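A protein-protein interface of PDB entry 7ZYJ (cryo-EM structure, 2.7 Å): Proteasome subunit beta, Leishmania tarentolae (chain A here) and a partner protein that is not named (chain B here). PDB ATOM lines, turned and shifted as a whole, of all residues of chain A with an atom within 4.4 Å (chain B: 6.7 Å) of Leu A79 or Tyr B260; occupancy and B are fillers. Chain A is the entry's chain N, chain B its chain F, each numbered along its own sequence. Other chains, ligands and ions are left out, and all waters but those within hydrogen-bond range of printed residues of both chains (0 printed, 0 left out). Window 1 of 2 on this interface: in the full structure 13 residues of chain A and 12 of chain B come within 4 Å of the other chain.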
ATOM      1  N   ASN A  66      -3.819   8.480 -20.986  1.00  0.00           N
ATOM      2  CA  ASN A  66      -4.754   9.453 -21.541  1.00  0.00           C
ATOM      3  C   ASN A  66      -5.545   8.886 -22.714  1.00  0.00           C
ATOM      4  O   ASN A  66      -6.748   9.145 -22.827  1.00  0.00           O
ATOM      5  CB  ASN A  66      -3.996  10.710 -21.968  1.00  0.00           C
ATOM      6  CG  ASN A  66      -4.920  11.835 -22.383  1.00  0.00           C
ATOM      7  OD1 ASN A  66      -5.116  12.085 -23.572  1.00  0.00           O
ATOM      8  ND2 ASN A  66      -5.490  12.524 -21.403  1.00  0.00           N
ATOM      9  N   ILE A  67      -4.895   8.124 -23.595  1.00  0.00           N
ATOM     10  CA  ILE A  67      -5.584   7.582 -24.764  1.00  0.00           C
ATOM     11  C   ILE A  67      -6.615   6.542 -24.343  1.00  0.00           C
ATOM     12  O   ILE A  67      -7.787   6.607 -24.738  1.00  0.00           O
ATOM     13  CB  ILE A  67      -4.567   6.985 -25.753  1.00  0.00           C
ATOM     14  CG1 ILE A  67      -3.561   8.044 -26.202  1.00  0.00           C
ATOM     15  CG2 ILE A  67      -5.279   6.382 -26.954  1.00  0.00           C
ATOM     16  CD1 ILE A  67      -2.419   7.477 -27.010  1.00  0.00           C
ATOM     17  N   GLN A  70      -9.627   7.969 -22.285  1.00  0.00           N
ATOM     18  CA  GLN A  70     -10.548   8.719 -23.133  1.00  0.00           C
ATOM     19  C   GLN A  70     -11.362   7.790 -24.023  1.00  0.00           C
ATOM     20  O   GLN A  70     -12.568   7.996 -24.208  1.00  0.00           O
ATOM     21  CB  GLN A  70      -9.787   9.735 -23.981  1.00  0.00           C
ATOM     22  CG  GLN A  70     -10.696  10.612 -24.825  1.00  0.00           C
ATOM     23  CD  GLN A  70      -9.936  11.653 -25.616  1.00  0.00           C
ATOM     24  OE1 GLN A  70      -8.708  11.709 -25.570  1.00  0.00           O
ATOM     25  NE2 GLN A  70     -10.664  12.482 -26.354  1.00  0.00           N
ATOM     26  N   ASP A  77     -14.078   8.101 -30.812  1.00  0.00           N
ATOM     27  CA  ASP A  77     -13.013   7.485 -31.583  1.00  0.00           C
ATOM     28  C   ASP A  77     -11.678   7.640 -30.862  1.00  0.00           C
ATOM     29  O   ASP A  77     -11.458   8.580 -30.094  1.00  0.00           O
ATOM     30  CB  ASP A  77     -12.929   8.102 -32.979  1.00  0.00           C
ATOM     31  CG  ASP A  77     -14.019   7.603 -33.902  1.00  0.00           C
ATOM     32  OD1 ASP A  77     -14.552   6.501 -33.655  1.00  0.00           O
ATOM     33  OD2 ASP A  77     -14.345   8.312 -34.878  1.00  0.00           O
ATOM     34  N   GLU A  78     -10.783   6.690 -31.114  1.00  0.00           N
ATOM     35  CA  GLU A  78      -9.448   6.755 -30.541  1.00  0.00           C
ATOM     36  C   GLU A  78      -8.693   7.956 -31.101  1.00  0.00           C
ATOM     37  O   GLU A  78      -8.889   8.359 -32.251  1.00  0.00           O
ATOM     38  CB  GLU A  78      -8.689   5.460 -30.830  1.00  0.00           C
ATOM     39  CG  GLU A  78      -7.334   5.356 -30.163  1.00  0.00           C
ATOM     40  CD  GLU A  78      -6.643   4.046 -30.468  1.00  0.00           C
ATOM     41  OE1 GLU A  78      -7.259   3.188 -31.134  1.00  0.00           O
ATOM     42  OE2 GLU A  78      -5.483   3.872 -30.048  1.00  0.00           O
ATOM     43  N   LEU A  79      -7.834   8.538 -30.267  1.00  0.00           N
ATOM     44  CA  LEU A  79      -7.097   9.731 -30.660  1.00  0.00           C
ATOM     45  C   LEU A  79      -6.241   9.466 -31.892  1.00  0.00           C
ATOM     46  O   LEU A  79      -5.599   8.419 -32.013  1.00  0.00           O
ATOM     47  CB  LEU A  79      -6.215  10.214 -29.509  1.00  0.00           C
ATOM     48  CG  LEU A  79      -6.892  10.956 -28.357  1.00  0.00           C
ATOM     49  CD1 LEU A  79      -5.929  11.105 -27.192  1.00  0.00           C
ATOM     50  CD2 LEU A  79      -7.399  12.311 -28.811  1.00  0.00           C
ATOM     51  N   SER A  80      -6.241  10.427 -32.810  1.00  0.00           N
ATOM     52  CA  SER A  80      -5.402  10.351 -33.990  1.00  0.00           C
ATOM     53  C   SER A  80      -3.937  10.522 -33.597  1.00  0.00           C
ATOM     54  O   SER A  80      -3.630  11.140 -32.575  1.00  0.00           O
ATOM     55  CB  SER A  80      -5.818  11.427 -34.992  1.00  0.00           C
ATOM     56  OG  SER A  80      -5.059  11.366 -36.185  1.00  0.00           O
ATOM     57  N   PRO A  81      -3.010   9.968 -34.387  1.00  0.00           N
ATOM     58  CA  PRO A  81      -1.582  10.160 -34.076  1.00  0.00           C
ATOM     59  C   PRO A  81      -1.176  11.621 -33.968  1.00  0.00           C
ATOM     60  O   PRO A  81      -0.340  11.966 -33.123  1.00  0.00           O
ATOM     61  CB  PRO A  81      -0.879   9.456 -35.244  1.00  0.00           C
ATOM     62  CG  PRO A  81      -1.844   8.416 -35.682  1.00  0.00           C
ATOM     63  CD  PRO A  81      -3.212   9.004 -35.483  1.00  0.00           C
ATOM     64  N   GLU A  83      -3.133  14.013 -32.866  1.00  0.00           N
ATOM     65  CA  GLU A  83      -3.638  14.458 -31.571  1.00  0.00           C
ATOM     66  C   GLU A  83      -2.788  13.919 -30.427  1.00  0.00           C
ATOM     67  O   GLU A  83      -2.533  14.631 -29.446  1.00  0.00           O
ATOM     68  CB  GLU A  83      -5.097  14.036 -31.409  1.00  0.00           C
ATOM     69  CG  GLU A  83      -6.023  14.646 -32.448  1.00  0.00           C
ATOM     70  CD  GLU A  83      -7.164  13.726 -32.829  1.00  0.00           C
ATOM     71  OE1 GLU A  83      -7.465  12.795 -32.054  1.00  0.00           O
ATOM     72  OE2 GLU A  83      -7.760  13.932 -33.906  1.00  0.00           O
ATOM     73  N   VAL A  84      -2.340  12.666 -30.533  1.00  0.00           N
ATOM     74  CA  VAL A  84      -1.470  12.100 -29.505  1.00  0.00           C
ATOM     75  C   VAL A  84      -0.161  12.871 -29.431  1.00  0.00           C
ATOM     76  O   VAL A  84       0.330  13.189 -28.340  1.00  0.00           O
ATOM     77  CB  VAL A  84      -1.230  10.601 -29.769  1.00  0.00           C
ATOM     78  CG1 VAL A  84      -0.375  10.004 -28.667  1.00  0.00           C
ATOM     79  CG2 VAL A  84      -2.551   9.864 -29.871  1.00  0.00           C
ATOM     80  N   ARG A 112      -2.943   6.259 -39.537  1.00  0.00           N
ATOM     81  CA  ARG A 112      -4.362   5.973 -39.381  1.00  0.00           C
ATOM     82  C   ARG A 112      -5.054   6.132 -40.725  1.00  0.00           C
ATOM     83  O   ARG A 112      -4.944   7.186 -41.356  1.00  0.00           O
ATOM     84  CB  ARG A 112      -5.019   6.890 -38.346  1.00  0.00           C
ATOM     85  CG  ARG A 112      -6.395   6.408 -37.912  1.00  0.00           C
ATOM     86  CD  ARG A 112      -7.031   7.334 -36.893  1.00  0.00           C
ATOM     87  NE  ARG A 112      -7.464   8.589 -37.495  1.00  0.00           N
ATOM     88  CZ  ARG A 112      -8.118   9.542 -36.847  1.00  0.00           C
ATOM     89  NH1 ARG A 112      -8.438   9.414 -35.571  1.00  0.00           N
ATOM     90  NH2 ARG A 112      -8.462  10.650 -37.497  1.00  0.00           N
ATOM     91  N   THR B 255     -14.664  27.439 -22.442  1.00  0.00           N
ATOM     92  CA  THR B 255     -13.375  27.220 -21.796  1.00  0.00           C
ATOM     93  C   THR B 255     -12.900  25.784 -21.982  1.00  0.00           C
ATOM     94  O   THR B 255     -11.724  25.544 -22.277  1.00  0.00           O
ATOM     95  CB  THR B 255     -13.465  27.566 -20.311  1.00  0.00           C
ATOM     96  OG1 THR B 255     -14.000  28.886 -20.158  1.00  0.00           O
ATOM     97  CG2 THR B 255     -12.089  27.507 -19.665  1.00  0.00           C
ATOM     98  N   GLU B 256     -13.806  24.816 -21.823  1.00  0.00           N
ATOM     99  CA  GLU B 256     -13.421  23.417 -21.990  1.00  0.00           C
ATOM    100  C   GLU B 256     -13.033  23.114 -23.433  1.00  0.00           C
ATOM    101  O   GLU B 256     -12.076  22.370 -23.680  1.00  0.00           O
ATOM    102  CB  GLU B 256     -14.553  22.501 -21.530  1.00  0.00           C
ATOM    103  CG  GLU B 256     -14.881  22.618 -20.051  1.00  0.00           C
ATOM    104  CD  GLU B 256     -13.666  22.447 -19.160  1.00  0.00           C
ATOM    105  OE1 GLU B 256     -12.813  21.587 -19.464  1.00  0.00           O
ATOM    106  OE2 GLU B 256     -13.561  23.175 -18.152  1.00  0.00           O
ATOM    107  N   CYS B 257     -13.761  23.679 -24.397  1.00  0.00           N
ATOM    108  CA  CYS B 257     -13.413  23.484 -25.800  1.00  0.00           C
ATOM    109  C   CYS B 257     -12.055  24.088 -26.122  1.00  0.00           C
ATOM    110  O   CYS B 257     -11.258  23.487 -26.852  1.00  0.00           O
ATOM    111  CB  CYS B 257     -14.487  24.095 -26.695  1.00  0.00           C
ATOM    112  SG  CYS B 257     -15.963  23.094 -26.854  1.00  0.00           S
ATOM    113  N   MET B 258     -11.777  25.281 -25.594  1.00  0.00           N
ATOM    114  CA  MET B 258     -10.480  25.905 -25.817  1.00  0.00           C
ATOM    115  C   MET B 258      -9.362  25.080 -25.194  1.00  0.00           C
ATOM    116  O   MET B 258      -8.288  24.930 -25.789  1.00  0.00           O
ATOM    117  CB  MET B 258     -10.484  27.325 -25.256  1.00  0.00           C
ATOM    118  CG  MET B 258     -11.068  28.358 -26.200  1.00  0.00           C
ATOM    119  SD  MET B 258     -11.023  30.027 -25.524  1.00  0.00           S
ATOM    120  CE  MET B 258     -12.591  30.664 -26.108  1.00  0.00           C
ATOM    121  N   ASN B 259      -9.595  24.541 -23.995  1.00  0.00           N
ATOM    122  CA  ASN B 259      -8.595  23.691 -23.359  1.00  0.00           C
ATOM    123  C   ASN B 259      -8.338  22.431 -24.178  1.00  0.00           C
ATOM    124  O   ASN B 259      -7.185  22.025 -24.358  1.00  0.00           O
ATOM    125  CB  ASN B 259      -9.041  23.323 -21.944  1.00  0.00           C
ATOM    126  CG  ASN B 259      -8.927  24.483 -20.973  1.00  0.00           C
ATOM    127  OD1 ASN B 259      -8.630  25.609 -21.370  1.00  0.00           O
ATOM    128  ND2 ASN B 259      -9.168  24.216 -19.695  1.00  0.00           N
ATOM    129  N   TYR B 260      -9.401  21.799 -24.680  1.00  0.00           N
ATOM    130  CA  TYR B 260      -9.235  20.567 -25.446  1.00  0.00           C
ATOM    131  C   TYR B 260      -8.514  20.827 -26.762  1.00  0.00           C
ATOM    132  O   TYR B 260      -7.568  20.115 -27.113  1.00  0.00           O
ATOM    133  CB  TYR B 260     -10.593  19.913 -25.695  1.00  0.00           C
ATOM    134  CG  TYR B 260     -10.512  18.554 -26.356  1.00  0.00           C
ATOM    135  CD1 TYR B 260     -10.377  18.433 -27.732  1.00  0.00           C
ATOM    136  CD2 TYR B 260     -10.569  17.390 -25.601  1.00  0.00           C
ATOM    137  CE1 TYR B 260     -10.298  17.196 -28.337  1.00  0.00           C
ATOM    138  CE2 TYR B 260     -10.494  16.147 -26.199  1.00  0.00           C
ATOM    139  CZ  TYR B 260     -10.358  16.057 -27.567  1.00  0.00           C
ATOM    140  OH  TYR B 260     -10.282  14.823 -28.170  1.00  0.00           O
ATOM    141  N   ARG B 261      -8.956  21.839 -27.514  1.00  0.00           N
ATOM    142  CA  ARG B 261      -8.330  22.134 -28.796  1.00  0.00           C
ATOM    143  C   ARG B 261      -6.878  22.559 -28.638  1.00  0.00           C
ATOM    144  O   ARG B 261      -6.095  22.422 -29.582  1.00  0.00           O
ATOM    145  CB  ARG B 261      -9.119  23.217 -29.531  1.00  0.00           C
ATOM    146  CG  ARG B 261      -8.789  23.325 -31.009  1.00  0.00           C
ATOM    147  CD  ARG B 261      -9.673  24.344 -31.702  1.00  0.00           C
ATOM    148  NE  ARG B 261     -11.010  23.826 -31.959  1.00  0.00           N
ATOM    149  CZ  ARG B 261     -11.328  23.050 -32.986  1.00  0.00           C
ATOM    150  NH1 ARG B 261     -10.422  22.665 -33.869  1.00  0.00           N
ATOM    151  NH2 ARG B 261     -12.587  22.649 -33.130  1.00  0.00           N
ATOM    152  N   TYR B 262      -6.502  23.070 -27.466  1.00  0.00           N
ATOM    153  CA  TYR B 262      -5.106  23.405 -27.221  1.00  0.00           C
ATOM    154  C   TYR B 262      -4.261  22.155 -27.004  1.00  0.00           C
ATOM    155  O   TYR B 262      -3.127  22.084 -27.488  1.00  0.00           O
ATOM    156  CB  TYR B 262      -5.005  24.346 -26.020  1.00  0.00           C
ATOM    157  CG  TYR B 262      -3.619  24.476 -25.437  1.00  0.00           C
ATOM    158  CD1 TYR B 262      -2.666  25.287 -26.036  1.00  0.00           C
ATOM    159  CD2 TYR B 262      -3.268  23.801 -24.276  1.00  0.00           C
ATOM    160  CE1 TYR B 262      -1.401  25.411 -25.503  1.00  0.00           C
ATOM    161  CE2 TYR B 262      -2.005  23.921 -23.737  1.00  0.00           C
ATOM    162  CZ  TYR B 262      -1.076  24.727 -24.353  1.00  0.00           C
ATOM    163  OH  TYR B 262       0.184  24.848 -23.817  1.00  0.00           O
ATOM    164  N   MET B 263      -4.793  21.164 -26.287  1.00  0.00           N
ATOM    165  CA  MET B 263      -4.018  19.969 -25.971  1.00  0.00           C
ATOM    166  C   MET B 263      -3.889  19.029 -27.164  1.00  0.00           C
ATOM    167  O   MET B 263      -2.826  18.434 -27.371  1.00  0.00           O
ATOM    168  CB  MET B 263      -4.650  19.236 -24.788  1.00  0.00           C
ATOM    169  CG  MET B 263      -4.711  20.051 -23.511  1.00  0.00           C
ATOM    170  SD  MET B 263      -3.086  20.569 -22.931  1.00  0.00           S
ATOM    171  CE  MET B 263      -2.270  18.985 -22.762  1.00  0.00           C
ATOM    172  N   TYR B 264      -4.945  18.882 -27.961  1.00  0.00           N
ATOM    173  CA  TYR B 264      -4.989  17.864 -29.003  1.00  0.00           C
ATOM    174  C   TYR B 264      -5.076  18.432 -30.412  1.00  0.00           C
ATOM    175  O   TYR B 264      -5.073  17.654 -31.373  1.00  0.00           O
ATOM    176  CB  TYR B 264      -6.169  16.915 -28.763  1.00  0.00           C
ATOM    177  CG  TYR B 264      -6.224  16.357 -27.361  1.00  0.00           C
ATOM    178  CD1 TYR B 264      -5.492  15.232 -27.012  1.00  0.00           C
ATOM    179  CD2 TYR B 264      -7.007  16.957 -26.386  1.00  0.00           C
ATOM    180  CE1 TYR B 264      -5.539  14.720 -25.732  1.00  0.00           C
ATOM    181  CE2 TYR B 264      -7.061  16.452 -25.103  1.00  0.00           C
ATOM    182  CZ  TYR B 264      -6.326  15.333 -24.782  1.00  0.00           C
ATOM    183  OH  TYR B 264      -6.377  14.827 -23.505  1.00  0.00           O
ATOM    184  N   SER B 265      -5.159  19.755 -30.562  1.00  0.00           N
ATOM    185  CA  SER B 265      -5.226  20.402 -31.874  1.00  0.00           C
ATOM    186  C   SER B 265      -6.426  19.911 -32.678  1.00  0.00           C
ATOM    187  O   SER B 265      -6.371  19.794 -33.903  1.00  0.00           O
ATOM    188  CB  SER B 265      -3.927  20.200 -32.659  1.00  0.00           C
ATOM    189  OG  SER B 265      -2.869  20.957 -32.100  1.00  0.00           O
ATOM    190  N   ASN B 266      -7.524  19.622 -31.984  1.00  0.00           N
ATOM    191  CA  ASN B 266      -8.739  19.156 -32.637  1.00  0.00           C
ATOM    192  C   ASN B 266      -9.925  19.455 -31.734  1.00  0.00           C
ATOM    193  O   ASN B 266      -9.771  19.702 -30.536  1.00  0.00           O
ATOM    194  CB  ASN B 266      -8.667  17.660 -32.962  1.00  0.00           C
ATOM    195  CG  ASN B 266      -9.650  17.252 -34.041  1.00  0.00           C
ATOM    196  OD1 ASN B 266     -10.098  18.081 -34.832  1.00  0.00           O
ATOM    197  ND2 ASN B 266      -9.991  15.970 -34.075  1.00  0.00           N
ATOM    198  N   GLY B 267     -11.114  19.431 -32.329  1.00  0.00           N
ATOM    199  CA  GLY B 267     -12.318  19.717 -31.575  1.00  0.00           C
ATOM    200  C   GLY B 267     -12.702  18.583 -30.644  1.00  0.00           C
ATOM    201  O   GLY B 267     -12.432  17.410 -30.902  1.00  0.00           O
ATOM    202  N   MET B 268     -13.347  18.950 -29.544  1.00  0.00           N
ATOM    203  CA  MET B 268     -13.790  17.959 -28.576  1.00  0.00           C
ATOM    204  C   MET B 268     -14.885  17.085 -29.181  1.00  0.00           C
ATOM    205  O   MET B 268     -15.795  17.598 -29.844  1.00  0.00           O
ATOM    206  CB  MET B 268     -14.309  18.643 -27.310  1.00  0.00           C
ATOM    207  CG  MET B 268     -14.684  17.683 -26.193  1.00  0.00           C
ATOM    208  SD  MET B 268     -15.281  18.524 -24.716  1.00  0.00           S
ATOM    209  CE  MET B 268     -13.763  19.238 -24.097  1.00  0.00           C
ATOM    210  N   PRO B 269     -14.827  15.770 -28.987  1.00  0.00           N
ATOM    211  CA  PRO B 269     -15.928  14.910 -29.434  1.00  0.00           C
ATOM    212  C   PRO B 269     -17.206  15.210 -28.670  1.00  0.00           C
ATOM    213  O   PRO B 269     -17.185  15.622 -27.508  1.00  0.00           O
ATOM    214  CB  PRO B 269     -15.421  13.493 -29.141  1.00  0.00           C
ATOM    215  CG  PRO B 269     -13.947  13.632 -28.930  1.00  0.00           C
ATOM    216  CD  PRO B 269     -13.733  14.999 -28.377  1.00  0.00           C
ATOM    217  N   GLN B 272     -18.060  13.103 -25.348  1.00  0.00           N
ATOM    218  CA  GLN B 272     -17.301  13.590 -24.203  1.00  0.00           C
ATOM    219  C   GLN B 272     -17.847  14.923 -23.713  1.00  0.00           C
ATOM    220  O   GLN B 272     -17.936  15.161 -22.503  1.00  0.00           O
ATOM    221  CB  GLN B 272     -15.824  13.717 -24.575  1.00  0.00           C
ATOM    222  CG  GLN B 272     -14.924  14.137 -23.429  1.00  0.00           C
ATOM    223  CD  GLN B 272     -13.467  14.204 -23.834  1.00  0.00           C
ATOM    224  OE1 GLN B 272     -13.101  13.819 -24.943  1.00  0.00           O
ATOM    225  NE2 GLN B 272     -12.624  14.694 -22.934  1.00  0.00           N
ATOM    226  N   MET B 276     -19.408  15.823 -20.064  1.00  0.00           N
ATOM    227  CA  MET B 276     -18.907  16.920 -19.241  1.00  0.00           C
ATOM    228  C   MET B 276     -20.036  17.841 -18.790  1.00  0.00           C
ATOM    229  O   MET B 276     -20.066  18.282 -17.636  1.00  0.00           O
ATOM    230  CB  MET B 276     -17.835  17.700 -20.000  1.00  0.00           C
ATOM    231  CG  MET B 276     -16.574  16.896 -20.252  1.00  0.00           C
ATOM    232  SD  MET B 276     -15.345  17.787 -21.216  1.00  0.00           S
ATOM    233  CE  MET B 276     -14.819  19.010 -20.022  1.00  0.00           C
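The side-chain hydroxyl of Tyr B264 lies within hydrogen-bond range of the side-chain amide oxygen of Asn A66 (3.0 Å).
The side-chain amide nitrogen (NE2) of Gln A70 sits at hydrogen-bond distance from the side-chain amide oxygen (OE1) of Gln B272 (3.1 Å).
The side-chain amide nitrogen (NE2) of Gln A70 is in hydrogen-bond range of the side-chain hydroxyl (OH) of Tyr B260, 3.0 Å away.
OE2 of Glu A83 sits at hydrogen-bond distance from ND2 of Asn B266.
OE1 of Glu A83 sits at hydrogen-bond distance from N of Ser A80, at 2.8 Å.
Leu A79 touches Tyr B260 (CD2 to OH, 3.9 Å).
Leu A79 touches Tyr B264 (CD1 to CE1, 3.9 Å).
Glu A83 touches Tyr B264 (CG to O, 3.3 Å).
Of the printed residues of chain B, Asn A66 touches Tyr B264.
Printed residues of chain B within 4 Å of Gln A70: Tyr B260 and Gln B272.
Of chain B, only Tyr B260 (3.9 Å) and Tyr B264 (3.9 Å) come within 4 Å of Leu A79.
Of the printed residues of chain B, Glu A83 touches Tyr B264 (3.3 Å) and Asn B266 (3.0 Å).
Tyr B260 touches two residues of chain A.
Of the printed residues of chain A, Asn B266 touches Glu A83 (3.0 Å).
Pro B269 touches none of the printed residues of chain A.
Of the printed residues of chain A, Gln B272 touches Gln A70.
The nearest printed residue of chain A that does not touch Asn B266 is Ser A80 (6.2 Å).
Along chain B the printed residues that touch a printed residue of chain A span positions 260 to 272.
Among the printed residues, 7 pairs touch across the chains.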
